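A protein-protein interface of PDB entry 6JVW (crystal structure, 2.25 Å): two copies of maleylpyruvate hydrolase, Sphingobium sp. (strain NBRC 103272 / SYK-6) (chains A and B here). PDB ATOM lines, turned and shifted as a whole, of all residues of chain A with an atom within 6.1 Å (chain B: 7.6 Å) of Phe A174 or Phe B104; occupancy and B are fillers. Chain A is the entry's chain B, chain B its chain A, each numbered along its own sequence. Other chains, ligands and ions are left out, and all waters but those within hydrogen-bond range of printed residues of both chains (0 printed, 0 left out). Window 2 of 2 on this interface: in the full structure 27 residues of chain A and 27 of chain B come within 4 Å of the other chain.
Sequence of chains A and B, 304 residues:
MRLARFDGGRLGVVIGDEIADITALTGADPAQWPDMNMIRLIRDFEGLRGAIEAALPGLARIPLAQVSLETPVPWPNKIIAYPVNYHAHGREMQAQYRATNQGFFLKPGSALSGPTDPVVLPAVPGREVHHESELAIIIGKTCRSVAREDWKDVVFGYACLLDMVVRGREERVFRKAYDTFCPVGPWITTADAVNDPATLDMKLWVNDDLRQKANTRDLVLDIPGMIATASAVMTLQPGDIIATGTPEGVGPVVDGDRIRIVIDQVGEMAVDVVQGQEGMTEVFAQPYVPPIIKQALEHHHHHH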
ATOM      1  N   VAL A 166      29.152   3.717 -32.613  1.00  0.00           N
ATOM      2  CA  VAL A 166      29.032   2.708 -31.528  1.00  0.00           C
ATOM      3  C   VAL A 166      27.516   2.458 -31.486  1.00  0.00           C
ATOM      4  O   VAL A 166      26.772   3.379 -31.352  1.00  0.00           O
ATOM      5  CB  VAL A 166      29.572   3.206 -30.180  1.00  0.00           C
ATOM      6  CG1 VAL A 166      29.521   2.106 -29.149  1.00  0.00           C
ATOM      7  CG2 VAL A 166      30.977   3.752 -30.287  1.00  0.00           C
ATOM      8  N   ARG A 172      21.778   7.922 -29.339  1.00  0.00           N
ATOM      9  CA  ARG A 172      22.674   8.712 -28.445  1.00  0.00           C
ATOM     10  C   ARG A 172      23.748   9.414 -29.285  1.00  0.00           C
ATOM     11  O   ARG A 172      24.539   8.709 -29.951  1.00  0.00           O
ATOM     12  CB  ARG A 172      23.341   7.811 -27.397  1.00  0.00           C
ATOM     13  CG  ARG A 172      22.373   7.046 -26.503  1.00  0.00           C
ATOM     14  CD  ARG A 172      21.696   7.912 -25.454  1.00  0.00           C
ATOM     15  NE  ARG A 172      20.941   7.106 -24.494  1.00  0.00           N
ATOM     16  CZ  ARG A 172      19.615   6.909 -24.494  1.00  0.00           C
ATOM     17  NH1 ARG A 172      18.837   7.471 -25.408  1.00  0.00           N
ATOM     18  NH2 ARG A 172      19.064   6.143 -23.566  1.00  0.00           N
ATOM     19  N   VAL A 173      23.798  10.748 -29.214  1.00  0.00           N
ATOM     20  CA  VAL A 173      24.731  11.629 -29.992  1.00  0.00           C
ATOM     21  C   VAL A 173      26.198  11.241 -29.735  1.00  0.00           C
ATOM     22  O   VAL A 173      26.969  11.162 -30.713  1.00  0.00           O
ATOM     23  CB  VAL A 173      24.503  13.112 -29.650  1.00  0.00           C
ATOM     24  CG1 VAL A 173      25.631  13.986 -30.177  1.00  0.00           C
ATOM     25  CG2 VAL A 173      23.143  13.612 -30.148  1.00  0.00           C
ATOM     26  N   PHE A 174      26.580  11.015 -28.473  1.00  0.00           N
ATOM     27  CA  PHE A 174      27.974  10.681 -28.092  1.00  0.00           C
ATOM     28  C   PHE A 174      28.453   9.484 -28.932  1.00  0.00           C
ATOM     29  O   PHE A 174      29.630   9.446 -29.233  1.00  0.00           O
ATOM     30  CB  PHE A 174      28.122  10.461 -26.579  1.00  0.00           C
ATOM     31  CG  PHE A 174      27.704   9.110 -26.047  1.00  0.00           C
ATOM     32  CD1 PHE A 174      28.531   8.001 -26.186  1.00  0.00           C
ATOM     33  CD2 PHE A 174      26.497   8.956 -25.375  1.00  0.00           C
ATOM     34  CE1 PHE A 174      28.141   6.760 -25.692  1.00  0.00           C
ATOM     35  CE2 PHE A 174      26.110   7.718 -24.877  1.00  0.00           C
ATOM     36  CZ  PHE A 174      26.935   6.623 -25.033  1.00  0.00           C
ATOM     37  N   ARG A 175      27.566   8.571 -29.324  1.00  0.00           N
ATOM     38  CA  ARG A 175      27.919   7.321 -30.053  1.00  0.00           C
ATOM     39  C   ARG A 175      28.443   7.599 -31.469  1.00  0.00           C
ATOM     40  O   ARG A 175      29.125   6.702 -31.998  1.00  0.00           O
ATOM     41  CB  ARG A 175      26.712   6.380 -30.119  1.00  0.00           C
ATOM     42  CG  ARG A 175      26.522   5.603 -28.829  1.00  0.00           C
ATOM     43  CD  ARG A 175      25.332   4.662 -28.855  1.00  0.00           C
ATOM     44  NE  ARG A 175      25.439   3.840 -27.665  1.00  0.00           N
ATOM     45  CZ  ARG A 175      24.430   3.450 -26.903  1.00  0.00           C
ATOM     46  NH1 ARG A 175      24.688   2.713 -25.837  1.00  0.00           N
ATOM     47  NH2 ARG A 175      23.181   3.784 -27.196  1.00  0.00           N
ATOM     48  N   LYS A 176      28.144   8.769 -32.053  1.00  0.00           N
ATOM     49  CA  LYS A 176      28.612   9.160 -33.413  1.00  0.00           C
ATOM     50  C   LYS A 176      29.751  10.179 -33.310  1.00  0.00           C
ATOM     51  O   LYS A 176      30.220  10.597 -34.378  1.00  0.00           O
ATOM     52  CB  LYS A 176      27.473   9.764 -34.247  1.00  0.00           C
ATOM     53  CG  LYS A 176      26.157   9.007 -34.176  1.00  0.00           C
ATOM     54  CD  LYS A 176      25.514   8.749 -35.505  1.00  0.00           C
ATOM     55  CE  LYS A 176      26.228   7.696 -36.330  1.00  0.00           C
ATOM     56  NZ  LYS A 176      25.375   7.168 -37.426  1.00  0.00           N
ATOM     57  N   ALA A 177      30.169  10.548 -32.089  1.00  0.00           N
ATOM     58  CA  ALA A 177      30.987  11.754 -31.828  1.00  0.00           C
ATOM     59  C   ALA A 177      32.459  11.444 -31.522  1.00  0.00           C
ATOM     60  O   ALA A 177      33.218  12.396 -31.523  1.00  0.00           O
ATOM     61  CB  ALA A 177      30.365  12.585 -30.725  1.00  0.00           C
ATOM     62  N   TYR A 178      32.863  10.193 -31.266  1.00  0.00           N
ATOM     63  CA  TYR A 178      34.266   9.837 -30.926  1.00  0.00           C
ATOM     64  C   TYR A 178      35.210  10.382 -32.024  1.00  0.00           C
ATOM     65  O   TYR A 178      34.846  10.418 -33.210  1.00  0.00           O
ATOM     66  CB  TYR A 178      34.399   8.327 -30.694  1.00  0.00           C
ATOM     67  CG  TYR A 178      33.801   7.845 -29.397  1.00  0.00           C
ATOM     68  CD1 TYR A 178      34.450   8.035 -28.186  1.00  0.00           C
ATOM     69  CD2 TYR A 178      32.567   7.211 -29.377  1.00  0.00           C
ATOM     70  CE1 TYR A 178      33.880   7.621 -26.992  1.00  0.00           C
ATOM     71  CE2 TYR A 178      31.981   6.795 -28.195  1.00  0.00           C
ATOM     72  CZ  TYR A 178      32.640   6.994 -26.995  1.00  0.00           C
ATOM     73  OH  TYR A 178      32.026   6.595 -25.833  1.00  0.00           O
ATOM     74  N   ILE B  79      29.647  23.173 -30.162  1.00  0.00           N
ATOM     75  CA  ILE B  79      28.829  23.608 -28.994  1.00  0.00           C
ATOM     76  C   ILE B  79      28.211  22.364 -28.358  1.00  0.00           C
ATOM     77  O   ILE B  79      27.379  21.702 -29.006  1.00  0.00           O
ATOM     78  CB  ILE B  79      27.738  24.614 -29.391  1.00  0.00           C
ATOM     79  CG1 ILE B  79      28.318  25.792 -30.166  1.00  0.00           C
ATOM     80  CG2 ILE B  79      26.979  25.074 -28.164  1.00  0.00           C
ATOM     81  CD1 ILE B  79      27.275  26.639 -30.832  1.00  0.00           C
ATOM     82  N   ILE B  80      28.671  22.015 -27.164  1.00  0.00           N
ATOM     83  CA  ILE B  80      28.236  20.786 -26.462  1.00  0.00           C
ATOM     84  C   ILE B  80      27.248  21.189 -25.383  1.00  0.00           C
ATOM     85  O   ILE B  80      27.582  22.073 -24.591  1.00  0.00           O
ATOM     86  CB  ILE B  80      29.443  20.071 -25.862  1.00  0.00           C
ATOM     87  CG1 ILE B  80      30.412  19.658 -26.968  1.00  0.00           C
ATOM     88  CG2 ILE B  80      28.982  18.884 -25.023  1.00  0.00           C
ATOM     89  CD1 ILE B  80      31.815  19.502 -26.479  1.00  0.00           C
ATOM     90  N   ALA B  81      26.068  20.601 -25.381  1.00  0.00           N
ATOM     91  CA  ALA B  81      24.988  21.031 -24.466  1.00  0.00           C
ATOM     92  C   ALA B  81      24.533  19.826 -23.636  1.00  0.00           C
ATOM     93  O   ALA B  81      24.378  18.713 -24.195  1.00  0.00           O
ATOM     94  CB  ALA B  81      23.858  21.658 -25.239  1.00  0.00           C
ATOM     95  N   TYR B  82      24.406  20.035 -22.332  1.00  0.00           N
ATOM     96  CA  TYR B  82      23.889  19.011 -21.394  1.00  0.00           C
ATOM     97  C   TYR B  82      22.401  19.248 -21.159  1.00  0.00           C
ATOM     98  O   TYR B  82      21.971  20.337 -20.774  1.00  0.00           O
ATOM     99  CB  TYR B  82      24.764  18.967 -20.147  1.00  0.00           C
ATOM    100  CG  TYR B  82      26.087  18.287 -20.389  1.00  0.00           C
ATOM    101  CD1 TYR B  82      26.232  16.918 -20.245  1.00  0.00           C
ATOM    102  CD2 TYR B  82      27.206  19.023 -20.764  1.00  0.00           C
ATOM    103  CE1 TYR B  82      27.461  16.292 -20.457  1.00  0.00           C
ATOM    104  CE2 TYR B  82      28.436  18.414 -20.978  1.00  0.00           C
ATOM    105  CZ  TYR B  82      28.569  17.045 -20.821  1.00  0.00           C
ATOM    106  OH  TYR B  82      29.788  16.464 -21.031  1.00  0.00           O
ATOM    107  N   PRO B  83      21.573  18.207 -21.364  1.00  0.00           N
ATOM    108  CA  PRO B  83      20.138  18.334 -21.141  1.00  0.00           C
ATOM    109  C   PRO B  83      19.866  18.235 -19.630  1.00  0.00           C
ATOM    110  O   PRO B  83      20.539  17.455 -18.987  1.00  0.00           O
ATOM    111  CB  PRO B  83      19.600  17.119 -21.904  1.00  0.00           C
ATOM    112  CG  PRO B  83      20.670  16.056 -21.661  1.00  0.00           C
ATOM    113  CD  PRO B  83      21.983  16.816 -21.640  1.00  0.00           C
ATOM    114  N   GLY B 103      22.745  11.642 -22.626  1.00  0.00           N
ATOM    115  CA  GLY B 103      24.043  12.347 -22.528  1.00  0.00           C
ATOM    116  C   GLY B 103      23.997  13.688 -23.241  1.00  0.00           C
ATOM    117  O   GLY B 103      22.876  14.147 -23.536  1.00  0.00           O
ATOM    118  N   PHE B 104      25.152  14.289 -23.561  1.00  0.00           N
ATOM    119  CA  PHE B 104      25.243  15.631 -24.214  1.00  0.00           C
ATOM    120  C   PHE B 104      24.718  15.586 -25.663  1.00  0.00           C
ATOM    121  O   PHE B 104      24.700  14.545 -26.314  1.00  0.00           O
ATOM    122  CB  PHE B 104      26.683  16.159 -24.191  1.00  0.00           C
ATOM    123  CG  PHE B 104      27.692  15.285 -24.897  1.00  0.00           C
ATOM    124  CD1 PHE B 104      27.886  15.385 -26.266  1.00  0.00           C
ATOM    125  CD2 PHE B 104      28.448  14.359 -24.190  1.00  0.00           C
ATOM    126  CE1 PHE B 104      28.815  14.587 -26.914  1.00  0.00           C
ATOM    127  CE2 PHE B 104      29.347  13.535 -24.846  1.00  0.00           C
ATOM    128  CZ  PHE B 104      29.536  13.657 -26.201  1.00  0.00           C
ATOM    129  N   PHE B 105      24.318  16.727 -26.192  1.00  0.00           N
ATOM    130  CA  PHE B 105      23.947  16.866 -27.621  1.00  0.00           C
ATOM    131  C   PHE B 105      24.779  18.018 -28.194  1.00  0.00           C
ATOM    132  O   PHE B 105      25.595  18.610 -27.475  1.00  0.00           O
ATOM    133  CB  PHE B 105      22.425  16.973 -27.773  1.00  0.00           C
ATOM    134  CG  PHE B 105      21.802  18.203 -27.168  1.00  0.00           C
ATOM    135  CD1 PHE B 105      21.664  19.362 -27.911  1.00  0.00           C
ATOM    136  CD2 PHE B 105      21.388  18.213 -25.841  1.00  0.00           C
ATOM    137  CE1 PHE B 105      21.099  20.501 -27.351  1.00  0.00           C
ATOM    138  CE2 PHE B 105      20.832  19.353 -25.274  1.00  0.00           C
ATOM    139  CZ  PHE B 105      20.691  20.501 -26.033  1.00  0.00           C
ATOM    140  N   LEU B 106      24.641  18.280 -29.482  1.00  0.00           N
ATOM    141  CA  LEU B 106      25.452  19.305 -30.177  1.00  0.00           C
ATOM    142  C   LEU B 106      24.502  20.358 -30.737  1.00  0.00           C
ATOM    143  O   LEU B 106      23.359  19.998 -31.098  1.00  0.00           O
ATOM    144  CB  LEU B 106      26.300  18.637 -31.261  1.00  0.00           C
ATOM    145  CG  LEU B 106      27.309  17.607 -30.754  1.00  0.00           C
ATOM    146  CD1 LEU B 106      27.826  16.750 -31.894  1.00  0.00           C
ATOM    147  CD2 LEU B 106      28.474  18.272 -30.034  1.00  0.00           C
ATOM    148  N   LEU B 221      25.352  16.877 -13.038  1.00  0.00           N
ATOM    149  CA  LEU B 221      26.727  16.597 -13.519  1.00  0.00           C
ATOM    150  C   LEU B 221      27.486  17.916 -13.428  1.00  0.00           C
ATOM    151  O   LEU B 221      27.082  18.870 -14.104  1.00  0.00           O
ATOM    152  CB  LEU B 221      26.678  16.047 -14.948  1.00  0.00           C
ATOM    153  CG  LEU B 221      28.020  15.611 -15.528  1.00  0.00           C
ATOM    154  CD1 LEU B 221      28.650  14.510 -14.690  1.00  0.00           C
ATOM    155  CD2 LEU B 221      27.861  15.143 -16.962  1.00  0.00           C
ATOM    156  N   MET B 226      31.287  17.494 -16.538  1.00  0.00           N
ATOM    157  CA  MET B 226      30.894  17.823 -17.934  1.00  0.00           C
ATOM    158  C   MET B 226      32.121  17.907 -18.862  1.00  0.00           C
ATOM    159  O   MET B 226      31.994  17.489 -20.019  1.00  0.00           O
ATOM    160  CB  MET B 226      30.083  19.122 -17.986  1.00  0.00           C
ATOM    161  CG  MET B 226      28.649  18.912 -17.537  1.00  0.00           C
ATOM    162  SD  MET B 226      27.695  20.432 -17.542  1.00  0.00           S
ATOM    163  CE  MET B 226      28.420  21.273 -16.141  1.00  0.00           C
ATOM    164  N   THR B 229      33.544  14.271 -19.244  1.00  0.00           N
ATOM    165  CA  THR B 229      32.623  13.472 -20.109  1.00  0.00           C
ATOM    166  C   THR B 229      32.817  13.867 -21.578  1.00  0.00           C
ATOM    167  O   THR B 229      33.084  12.995 -22.402  1.00  0.00           O
ATOM    168  CB  THR B 229      31.162  13.673 -19.696  1.00  0.00           C
ATOM    169  OG1 THR B 229      31.069  13.175 -18.363  1.00  0.00           O
ATOM    170  CG2 THR B 229      30.184  12.959 -20.602  1.00  0.00           C
ATOM    171  N   ALA B 230      32.763  15.158 -21.877  1.00  0.00           N
ATOM    172  CA  ALA B 230      32.890  15.683 -23.254  1.00  0.00           C
ATOM    173  C   ALA B 230      34.254  15.292 -23.856  1.00  0.00           C
ATOM    174  O   ALA B 230      34.248  14.794 -24.995  1.00  0.00           O
ATOM    175  CB  ALA B 230      32.679  17.180 -23.234  1.00  0.00           C
ATOM    176  N   SER B 231      35.358  15.539 -23.130  1.00  0.00           N
ATOM    177  CA  SER B 231      36.770  15.279 -23.541  1.00  0.00           C
ATOM    178  C   SER B 231      37.079  13.772 -23.646  1.00  0.00           C
ATOM    179  O   SER B 231      38.052  13.434 -24.313  1.00  0.00           O
ATOM    180  CB  SER B 231      37.750  15.954 -22.600  1.00  0.00           C
ATOM    181  OG  SER B 231      37.788  15.280 -21.342  1.00  0.00           O
ATOM    182  N   ALA B 232      36.289  12.891 -23.015  1.00  0.00           N
ATOM    183  CA  ALA B 232      36.462  11.426 -23.145  1.00  0.00           C
ATOM    184  C   ALA B 232      35.996  10.990 -24.538  1.00  0.00           C
ATOM    185  O   ALA B 232      36.483   9.963 -25.033  1.00  0.00           O
ATOM    186  CB  ALA B 232      35.695  10.701 -22.057  1.00  0.00           C
ATOM    187  N   VAL B 233      35.056  11.713 -25.141  1.00  0.00           N
ATOM    188  CA  VAL B 233      34.526  11.352 -26.479  1.00  0.00           C
ATOM    189  C   VAL B 233      35.305  12.145 -27.551  1.00  0.00           C
ATOM    190  O   VAL B 233      35.724  11.555 -28.550  1.00  0.00           O
ATOM    191  CB  VAL B 233      33.005  11.561 -26.536  1.00  0.00           C
ATOM    192  CG1 VAL B 233      32.456  11.145 -27.886  1.00  0.00           C
ATOM    193  CG2 VAL B 233      32.281  10.808 -25.413  1.00  0.00           C
ATOM    194  N   MET B 234      35.582  13.418 -27.317  1.00  0.00           N
ATOM    195  CA  MET B 234      36.007  14.379 -28.368  1.00  0.00           C
ATOM    196  C   MET B 234      37.247  15.143 -27.929  1.00  0.00           C
ATOM    197  O   MET B 234      37.303  15.555 -26.766  1.00  0.00           O
ATOM    198  CB  MET B 234      34.893  15.404 -28.609  1.00  0.00           C
ATOM    199  CG  MET B 234      33.565  14.784 -29.064  1.00  0.00           C
ATOM    200  SD  MET B 234      32.234  15.998 -29.108  1.00  0.00           S
ATOM    201  CE  MET B 234      32.076  16.328 -27.359  1.00  0.00           C
ATOM    202  N   ILE B 242      30.606  24.822 -23.904  1.00  0.00           N
ATOM    203  CA  ILE B 242      29.786  23.838 -23.147  1.00  0.00           C
ATOM    204  C   ILE B 242      28.647  24.582 -22.424  1.00  0.00           C
ATOM    205  O   ILE B 242      28.895  25.393 -21.515  1.00  0.00           O
ATOM    206  CB  ILE B 242      30.645  23.002 -22.198  1.00  0.00           C
ATOM    207  CG1 ILE B 242      31.759  22.267 -22.960  1.00  0.00           C
ATOM    208  CG2 ILE B 242      29.731  22.047 -21.448  1.00  0.00           C
ATOM    209  CD1 ILE B 242      32.655  21.432 -22.093  1.00  0.00           C
ATOM    210  N   ALA B 243      27.429  24.324 -22.884  1.00  0.00           N
ATOM    211  CA  ALA B 243      26.156  24.753 -22.290  1.00  0.00           C
ATOM    212  C   ALA B 243      25.843  23.796 -21.140  1.00  0.00           C
ATOM    213  O   ALA B 243      25.666  22.631 -21.413  1.00  0.00           O
ATOM    214  CB  ALA B 243      25.120  24.713 -23.380  1.00  0.00           C
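Phe B104 touches Val A173.
Val A173 touches Leu B106 (CG1 to CD1, 3.9 Å).
CZ of Phe B104 touches CB of Phe A174, 3.5 Å away.
Phe A174 touches Val B233 (O to CG1, 3.6 Å).
C of Ala A177 touches CG1 of Val B233 (3.6 Å).
Ala A177 touches Met B234.
Tyr A178 touches Val B233 (CA to O, 3.3 Å).
Of chain A, only Val A173 and Phe A174 come within 4 Å of Phe B104.
Of the printed residues of chain A, Leu B106 touches Val A173.
Of the printed residues of chain B, Val A173 touches Phe B104 and Leu B106.
The nearest residue of chain B that does not touch Phe A174 is Gly B103 (5.1 Å).
Printed residues of chain A that touch a printed residue of chain B: Val A173, Phe A174, Ala A177 and Tyr A178.
Of the 19 printed residues of chain B, 4 touch a printed residue of chain A.
Hydrophobic or aromatic side chains of chain B within 4 Å of the printed part of chain A: Phe B104, Leu B106, Val B233 and Met B234.
Among the printed residues, no Asp or Glu carboxylate lies within 4 Å of a Lys or Arg side-chain nitrogen of the other chain.
No position is printed for both chains.
Of the 7 pairs that touch across the chains among the printed residues, none has its exchanged pair printed and touching as well.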
